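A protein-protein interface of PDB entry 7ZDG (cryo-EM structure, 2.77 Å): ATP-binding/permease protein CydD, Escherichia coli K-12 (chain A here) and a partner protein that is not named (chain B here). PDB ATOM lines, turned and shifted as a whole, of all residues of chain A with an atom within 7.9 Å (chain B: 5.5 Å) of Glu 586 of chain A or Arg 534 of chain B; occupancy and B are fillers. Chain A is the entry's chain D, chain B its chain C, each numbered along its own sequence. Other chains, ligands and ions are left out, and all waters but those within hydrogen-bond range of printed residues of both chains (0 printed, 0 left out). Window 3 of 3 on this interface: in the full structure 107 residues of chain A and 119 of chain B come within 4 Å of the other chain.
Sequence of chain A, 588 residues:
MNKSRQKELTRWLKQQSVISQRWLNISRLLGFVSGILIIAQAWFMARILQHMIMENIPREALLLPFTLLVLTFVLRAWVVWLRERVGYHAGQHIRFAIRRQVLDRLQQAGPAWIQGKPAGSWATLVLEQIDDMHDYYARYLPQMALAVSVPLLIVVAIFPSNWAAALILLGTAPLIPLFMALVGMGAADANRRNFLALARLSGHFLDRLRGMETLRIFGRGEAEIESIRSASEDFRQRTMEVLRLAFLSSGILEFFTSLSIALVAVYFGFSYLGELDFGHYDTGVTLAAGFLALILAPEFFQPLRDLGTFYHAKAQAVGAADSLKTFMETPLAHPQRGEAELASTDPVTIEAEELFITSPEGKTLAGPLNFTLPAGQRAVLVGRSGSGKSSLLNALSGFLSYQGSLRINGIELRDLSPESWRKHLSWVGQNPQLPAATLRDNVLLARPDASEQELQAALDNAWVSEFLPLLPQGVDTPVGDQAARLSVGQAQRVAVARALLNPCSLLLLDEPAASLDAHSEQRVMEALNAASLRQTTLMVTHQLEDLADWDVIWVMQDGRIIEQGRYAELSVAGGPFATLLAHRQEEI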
ATOM      1  N   THR A 579       6.575 -18.819   7.180  1.00  0.00           N
ATOM      2  CA  THR A 579       6.820 -18.713   8.614  1.00  0.00           C
ATOM      3  C   THR A 579       5.599 -19.152   9.411  1.00  0.00           C
ATOM      4  O   THR A 579       5.715 -19.896  10.391  1.00  0.00           O
ATOM      5  CB  THR A 579       7.206 -17.279   8.971  1.00  0.00           C
ATOM      6  OG1 THR A 579       8.430 -16.936   8.312  1.00  0.00           O
ATOM      7  CG2 THR A 579       7.379 -17.130  10.470  1.00  0.00           C
ATOM      8  N   LEU A 580       4.412 -18.698   9.001  1.00  0.00           N
ATOM      9  CA  LEU A 580       3.184 -19.101   9.677  1.00  0.00           C
ATOM     10  C   LEU A 580       2.897 -20.579   9.469  1.00  0.00           C
ATOM     11  O   LEU A 580       2.442 -21.263  10.391  1.00  0.00           O
ATOM     12  CB  LEU A 580       2.016 -18.257   9.178  1.00  0.00           C
ATOM     13  CG  LEU A 580       1.961 -16.822   9.687  1.00  0.00           C
ATOM     14  CD1 LEU A 580       0.938 -16.039   8.902  1.00  0.00           C
ATOM     15  CD2 LEU A 580       1.632 -16.804  11.161  1.00  0.00           C
ATOM     16  N   LEU A 581       3.139 -21.086   8.261  1.00  0.00           N
ATOM     17  CA  LEU A 581       2.927 -22.505   8.000  1.00  0.00           C
ATOM     18  C   LEU A 581       3.865 -23.363   8.836  1.00  0.00           C
ATOM     19  O   LEU A 581       3.457 -24.399   9.371  1.00  0.00           O
ATOM     20  CB  LEU A 581       3.115 -22.798   6.515  1.00  0.00           C
ATOM     21  CG  LEU A 581       2.864 -24.238   6.089  1.00  0.00           C
ATOM     22  CD1 LEU A 581       1.428 -24.632   6.350  1.00  0.00           C
ATOM     23  CD2 LEU A 581       3.202 -24.401   4.625  1.00  0.00           C
ATOM     24  N   ALA A 582       5.129 -22.954   8.952  1.00  0.00           N
ATOM     25  CA  ALA A 582       6.068 -23.693   9.788  1.00  0.00           C
ATOM     26  C   ALA A 582       5.649 -23.655  11.249  1.00  0.00           C
ATOM     27  O   ALA A 582       5.724 -24.668  11.951  1.00  0.00           O
ATOM     28  CB  ALA A 582       7.475 -23.127   9.617  1.00  0.00           C
ATOM     29  N   HIS A 583       5.202 -22.491  11.723  1.00  0.00           N
ATOM     30  CA  HIS A 583       4.718 -22.378  13.094  1.00  0.00           C
ATOM     31  C   HIS A 583       3.488 -23.246  13.319  1.00  0.00           C
ATOM     32  O   HIS A 583       3.350 -23.878  14.371  1.00  0.00           O
ATOM     33  CB  HIS A 583       4.412 -20.916  13.412  1.00  0.00           C
ATOM     34  CG  HIS A 583       3.690 -20.710  14.707  1.00  0.00           C
ATOM     35  ND1 HIS A 583       2.318 -20.770  14.811  1.00  0.00           N
ATOM     36  CD2 HIS A 583       4.151 -20.425  15.947  1.00  0.00           C
ATOM     37  CE1 HIS A 583       1.964 -20.543  16.063  1.00  0.00           C
ATOM     38  NE2 HIS A 583       3.057 -20.330  16.772  1.00  0.00           N
ATOM     39  N   ARG A 584       2.580 -23.284  12.346  1.00  0.00           N
ATOM     40  CA  ARG A 584       1.404 -24.139  12.462  1.00  0.00           C
ATOM     41  C   ARG A 584       1.778 -25.613  12.497  1.00  0.00           C
ATOM     42  O   ARG A 584       1.185 -26.382  13.258  1.00  0.00           O
ATOM     43  CB  ARG A 584       0.443 -23.861  11.309  1.00  0.00           C
ATOM     44  CG  ARG A 584      -0.678 -24.869  11.163  1.00  0.00           C
ATOM     45  CD  ARG A 584      -1.605 -24.873  12.355  1.00  0.00           C
ATOM     46  NE  ARG A 584      -2.667 -25.858  12.191  1.00  0.00           N
ATOM     47  CZ  ARG A 584      -3.569 -26.145  13.120  1.00  0.00           C
ATOM     48  NH1 ARG A 584      -3.544 -25.518  14.285  1.00  0.00           N
ATOM     49  NH2 ARG A 584      -4.500 -27.057  12.882  1.00  0.00           N
ATOM     50  N   GLN A 585       2.749 -26.027  11.682  1.00  0.00           N
ATOM     51  CA  GLN A 585       3.142 -27.430  11.654  1.00  0.00           C
ATOM     52  C   GLN A 585       3.762 -27.886  12.966  1.00  0.00           C
ATOM     53  O   GLN A 585       3.797 -29.091  13.232  1.00  0.00           O
ATOM     54  CB  GLN A 585       4.118 -27.681  10.504  1.00  0.00           C
ATOM     55  CG  GLN A 585       3.502 -27.541   9.123  1.00  0.00           C
ATOM     56  CD  GLN A 585       2.751 -28.779   8.681  1.00  0.00           C
ATOM     57  OE1 GLN A 585       2.382 -29.622   9.495  1.00  0.00           O
ATOM     58  NE2 GLN A 585       2.515 -28.891   7.379  1.00  0.00           N
ATOM     59  N   GLU A 586       4.250 -26.957  13.791  1.00  0.00           N
ATOM     60  CA  GLU A 586       4.840 -27.346  15.066  1.00  0.00           C
ATOM     61  C   GLU A 586       3.784 -27.793  16.066  1.00  0.00           C
ATOM     62  O   GLU A 586       4.125 -28.440  17.058  1.00  0.00           O
ATOM     63  CB  GLU A 586       5.655 -26.195  15.647  1.00  0.00           C
ATOM     64  CG  GLU A 586       6.876 -25.837  14.823  1.00  0.00           C
ATOM     65  CD  GLU A 586       7.921 -26.930  14.805  1.00  0.00           C
ATOM     66  OE1 GLU A 586       8.041 -27.660  15.808  1.00  0.00           O
ATOM     67  OE2 GLU A 586       8.619 -27.068  13.781  1.00  0.00           O
ATOM     68  N   GLU A 587       2.519 -27.456  15.832  1.00  0.00           N
ATOM     69  CA  GLU A 587       1.434 -28.073  16.580  1.00  0.00           C
ATOM     70  C   GLU A 587       1.367 -29.553  16.245  1.00  0.00           C
ATOM     71  O   GLU A 587       1.805 -29.984  15.175  1.00  0.00           O
ATOM     72  CB  GLU A 587       0.102 -27.407  16.241  1.00  0.00           C
ATOM     73  CG  GLU A 587      -0.125 -26.058  16.885  1.00  0.00           C
ATOM     74  CD  GLU A 587      -0.664 -26.175  18.292  1.00  0.00           C
ATOM     75  OE1 GLU A 587      -1.390 -27.151  18.569  1.00  0.00           O
ATOM     76  OE2 GLU A 587      -0.371 -25.287  19.120  1.00  0.00           O
ATOM     77  N   ILE A 588       0.834 -30.330  17.191  1.00  0.00           N
ATOM     78  CA  ILE A 588       0.693 -31.809  17.035  1.00  0.00           C
ATOM     79  C   ILE A 588      -0.653 -32.105  16.363  1.00  0.00           C
ATOM     80  O   ILE A 588      -1.466 -32.796  17.007  1.00  0.00           O
ATOM     81  CB  ILE A 588       0.811 -32.516  18.398  1.00  0.00           C
ATOM     82  CG1 ILE A 588       2.138 -32.197  19.090  1.00  0.00           C
ATOM     83  CG2 ILE A 588       0.604 -34.015  18.250  1.00  0.00           C
ATOM     84  CD1 ILE A 588       2.366 -32.978  20.362  1.00  0.00           C
ATOM     85  N   ALA B 507       5.348 -17.073  16.750  1.00  0.00           N
ATOM     86  CA  ALA B 507       6.625 -17.776  16.696  1.00  0.00           C
ATOM     87  C   ALA B 507       7.744 -16.949  17.312  1.00  0.00           C
ATOM     88  O   ALA B 507       8.704 -17.501  17.860  1.00  0.00           O
ATOM     89  CB  ALA B 507       6.960 -18.143  15.253  1.00  0.00           C
ATOM     90  N   GLU B 510       7.117 -17.154  21.189  1.00  0.00           N
ATOM     91  CA  GLU B 510       7.296 -18.534  21.625  1.00  0.00           C
ATOM     92  C   GLU B 510       8.770 -18.902  21.703  1.00  0.00           C
ATOM     93  O   GLU B 510       9.186 -19.638  22.603  1.00  0.00           O
ATOM     94  CB  GLU B 510       6.556 -19.472  20.676  1.00  0.00           C
ATOM     95  CG  GLU B 510       6.824 -20.940  20.901  1.00  0.00           C
ATOM     96  CD  GLU B 510       6.450 -21.781  19.702  1.00  0.00           C
ATOM     97  OE1 GLU B 510       5.986 -22.923  19.896  1.00  0.00           O
ATOM     98  OE2 GLU B 510       6.624 -21.304  18.562  1.00  0.00           O
ATOM     99  N   SER B 511       9.575 -18.403  20.767  1.00  0.00           N
ATOM    100  CA  SER B 511      11.002 -18.703  20.789  1.00  0.00           C
ATOM    101  C   SER B 511      11.702 -18.000  21.945  1.00  0.00           C
ATOM    102  O   SER B 511      12.598 -18.573  22.573  1.00  0.00           O
ATOM    103  CB  SER B 511      11.637 -18.313  19.458  1.00  0.00           C
ATOM    104  OG  SER B 511      11.593 -16.911  19.268  1.00  0.00           O
ATOM    105  N   LEU B 514      10.780 -19.797  25.323  1.00  0.00           N
ATOM    106  CA  LEU B 514      11.439 -21.094  25.442  1.00  0.00           C
ATOM    107  C   LEU B 514      12.911 -20.933  25.792  1.00  0.00           C
ATOM    108  O   LEU B 514      13.451 -21.697  26.599  1.00  0.00           O
ATOM    109  CB  LEU B 514      11.282 -21.881  24.145  1.00  0.00           C
ATOM    110  CG  LEU B 514       9.996 -22.686  24.017  1.00  0.00           C
ATOM    111  CD1 LEU B 514       9.989 -23.444  22.710  1.00  0.00           C
ATOM    112  CD2 LEU B 514       9.857 -23.633  25.186  1.00  0.00           C
ATOM    113  N   HIS B 531       1.573 -29.339  23.783  1.00  0.00           N
ATOM    114  CA  HIS B 531       1.298 -30.036  22.541  1.00  0.00           C
ATOM    115  C   HIS B 531       1.974 -29.359  21.358  1.00  0.00           C
ATOM    116  O   HIS B 531       1.483 -29.475  20.231  1.00  0.00           O
ATOM    117  CB  HIS B 531      -0.210 -30.131  22.311  1.00  0.00           C
ATOM    118  CG  HIS B 531      -0.922 -28.821  22.421  1.00  0.00           C
ATOM    119  ND1 HIS B 531      -1.897 -28.584  23.364  1.00  0.00           N
ATOM    120  CD2 HIS B 531      -0.802 -27.677  21.709  1.00  0.00           C
ATOM    121  CE1 HIS B 531      -2.351 -27.352  23.224  1.00  0.00           C
ATOM    122  NE2 HIS B 531      -1.702 -26.780  22.228  1.00  0.00           N
ATOM    123  N   ARG B 532       3.073 -28.648  21.587  1.00  0.00           N
ATOM    124  CA  ARG B 532       3.837 -27.987  20.540  1.00  0.00           C
ATOM    125  C   ARG B 532       5.250 -28.553  20.513  1.00  0.00           C
ATOM    126  O   ARG B 532       5.849 -28.783  21.566  1.00  0.00           O
ATOM    127  CB  ARG B 532       3.876 -26.476  20.763  1.00  0.00           C
ATOM    128  CG  ARG B 532       2.529 -25.802  20.629  1.00  0.00           C
ATOM    129  CD  ARG B 532       2.690 -24.312  20.411  1.00  0.00           C
ATOM    130  NE  ARG B 532       3.754 -24.009  19.463  1.00  0.00           N
ATOM    131  CZ  ARG B 532       3.588 -23.927  18.148  1.00  0.00           C
ATOM    132  NH1 ARG B 532       2.393 -24.124  17.614  1.00  0.00           N
ATOM    133  NH2 ARG B 532       4.620 -23.645  17.368  1.00  0.00           N
ATOM    134  N   LEU B 533       5.779 -28.764  19.308  1.00  0.00           N
ATOM    135  CA  LEU B 533       7.061 -29.432  19.122  1.00  0.00           C
ATOM    136  C   LEU B 533       8.260 -28.505  19.271  1.00  0.00           C
ATOM    137  O   LEU B 533       9.395 -28.982  19.206  1.00  0.00           O
ATOM    138  CB  LEU B 533       7.115 -30.085  17.739  1.00  0.00           C
ATOM    139  CG  LEU B 533       6.487 -31.459  17.498  1.00  0.00           C
ATOM    140  CD1 LEU B 533       7.185 -32.503  18.325  1.00  0.00           C
ATOM    141  CD2 LEU B 533       4.997 -31.468  17.773  1.00  0.00           C
ATOM    142  N   ARG B 534       8.046 -27.208  19.456  1.00  0.00           N
ATOM    143  CA  ARG B 534       9.150 -26.258  19.421  1.00  0.00           C
ATOM    144  C   ARG B 534      10.048 -26.383  20.645  1.00  0.00           C
ATOM    145  O   ARG B 534       9.575 -26.547  21.771  1.00  0.00           O
ATOM    146  CB  ARG B 534       8.617 -24.831  19.325  1.00  0.00           C
ATOM    147  CG  ARG B 534       8.576 -24.282  17.918  1.00  0.00           C
ATOM    148  CD  ARG B 534       9.970 -24.220  17.330  1.00  0.00           C
ATOM    149  NE  ARG B 534      10.894 -23.504  18.202  1.00  0.00           N
ATOM    150  CZ  ARG B 534      10.976 -22.181  18.279  1.00  0.00           C
ATOM    151  NH1 ARG B 534      10.188 -21.423  17.531  1.00  0.00           N
ATOM    152  NH2 ARG B 534      11.848 -21.618  19.103  1.00  0.00           N
ATOM    153  N   GLY B 535      11.355 -26.290  20.414  1.00  0.00           N
ATOM    154  CA  GLY B 535      12.313 -26.146  21.497  1.00  0.00           C
ATOM    155  C   GLY B 535      12.468 -27.359  22.382  1.00  0.00           C
ATOM    156  O   GLY B 535      12.954 -27.234  23.510  1.00  0.00           O
ATOM    157  N   LEU B 536      12.083 -28.535  21.901  1.00  0.00           N
ATOM    158  CA  LEU B 536      12.171 -29.742  22.707  1.00  0.00           C
ATOM    159  C   LEU B 536      13.537 -30.404  22.645  1.00  0.00           C
ATOM    160  O   LEU B 536      13.747 -31.413  23.323  1.00  0.00           O
ATOM    161  CB  LEU B 536      11.105 -30.745  22.272  1.00  0.00           C
ATOM    162  CG  LEU B 536       9.666 -30.355  22.586  1.00  0.00           C
ATOM    163  CD1 LEU B 536       8.784 -31.564  22.475  1.00  0.00           C
ATOM    164  CD2 LEU B 536       9.567 -29.750  23.961  1.00  0.00           C
ATOM    165  N   LYS B 570       7.234 -34.851  13.629  1.00  0.00           N
ATOM    166  CA  LYS B 570       8.275 -33.995  12.997  1.00  0.00           C
ATOM    167  C   LYS B 570       8.128 -34.029  11.473  1.00  0.00           C
ATOM    168  O   LYS B 570       8.827 -33.249  10.798  1.00  0.00           O
ATOM    169  CB  LYS B 570       9.672 -34.451  13.427  1.00  0.00           C
ATOM    170  CG  LYS B 570       9.914 -34.467  14.930  1.00  0.00           C
ATOM    171  CD  LYS B 570       9.794 -33.102  15.571  1.00  0.00           C
ATOM    172  CE  LYS B 570      10.880 -32.144  15.133  1.00  0.00           C
ATOM    173  NZ  LYS B 570      10.765 -30.837  15.822  1.00  0.00           N
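OE2 of Glu 510 of chain B is in salt-bridge range of NH1 of Arg 534 of chain B, 3.7 Å away. NE of Arg 532 of chain B is in salt-bridge range of OE1 of Glu 510 of chain B (2.5 Å). The backbone carbonyl oxygen (O) of Ala 507 of chain B is in hydrogen-bond range of the side-chain hydroxyl (OG) of Ser 511 of chain B.
Printed residues of chain A that touch a printed residue of chain B: His 583, Glu 586, Glu 587 and Ile 588. Among the printed residues, 10 pairs touch across the chains.
N of Ala 507 of chain B touches CD2 of His 583 of chain A, 3.6 Å away. His 583 of chain A touches Glu 510 of chain B. CB of Glu 586 of chain A touches NH2 of Arg 532 of chain B (3.2 Å). N of Arg 534 of chain B touches OE1 of Glu 586 of chain A (3.7 Å). Glu 587 of chain A touches His 531 of chain B (OE1 to CD2, 3.2 Å). Ile 588 of chain A touches Leu 533 of chain B.
Of the printed residues of chain B, Glu 586 of chain A touches Arg 532 (3.2 Å), Leu 533 (2.8 Å) and Arg 534 (3.7 Å). Printed residues of chain A within 4 Å of Arg 532 of chain B: His 583 (3.3 Å), Glu 586 (3.2 Å) and Glu 587 (3.3 Å). Of the printed residues of chain A, Leu 533 of chain B touches Glu 586 and Ile 588. Arg 534 of chain B touches just one residue of chain A: Glu 586 (3.7 Å). The nearest residue of chain A that does not touch Arg 534 of chain B is His 583 of chain A (6.2 Å).
O of His 531 of chain B lies close to N of Ile 588 of chain A (3.2 Å). N of Leu 533 of chain B is in hydrogen-bond range of O of Glu 586 of chain A (2.8 Å). The guanidinium group (NH1) of Arg 532 of chain B is in salt-bridge range of the side-chain carboxylate (OE2) of Glu 587 of chain A (3.4 Å). The guanidinium group of Arg 532 of chain B sits at hydrogen-bond distance from the backbone carbonyl oxygen of His 583 of chain A (3.3 Å).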
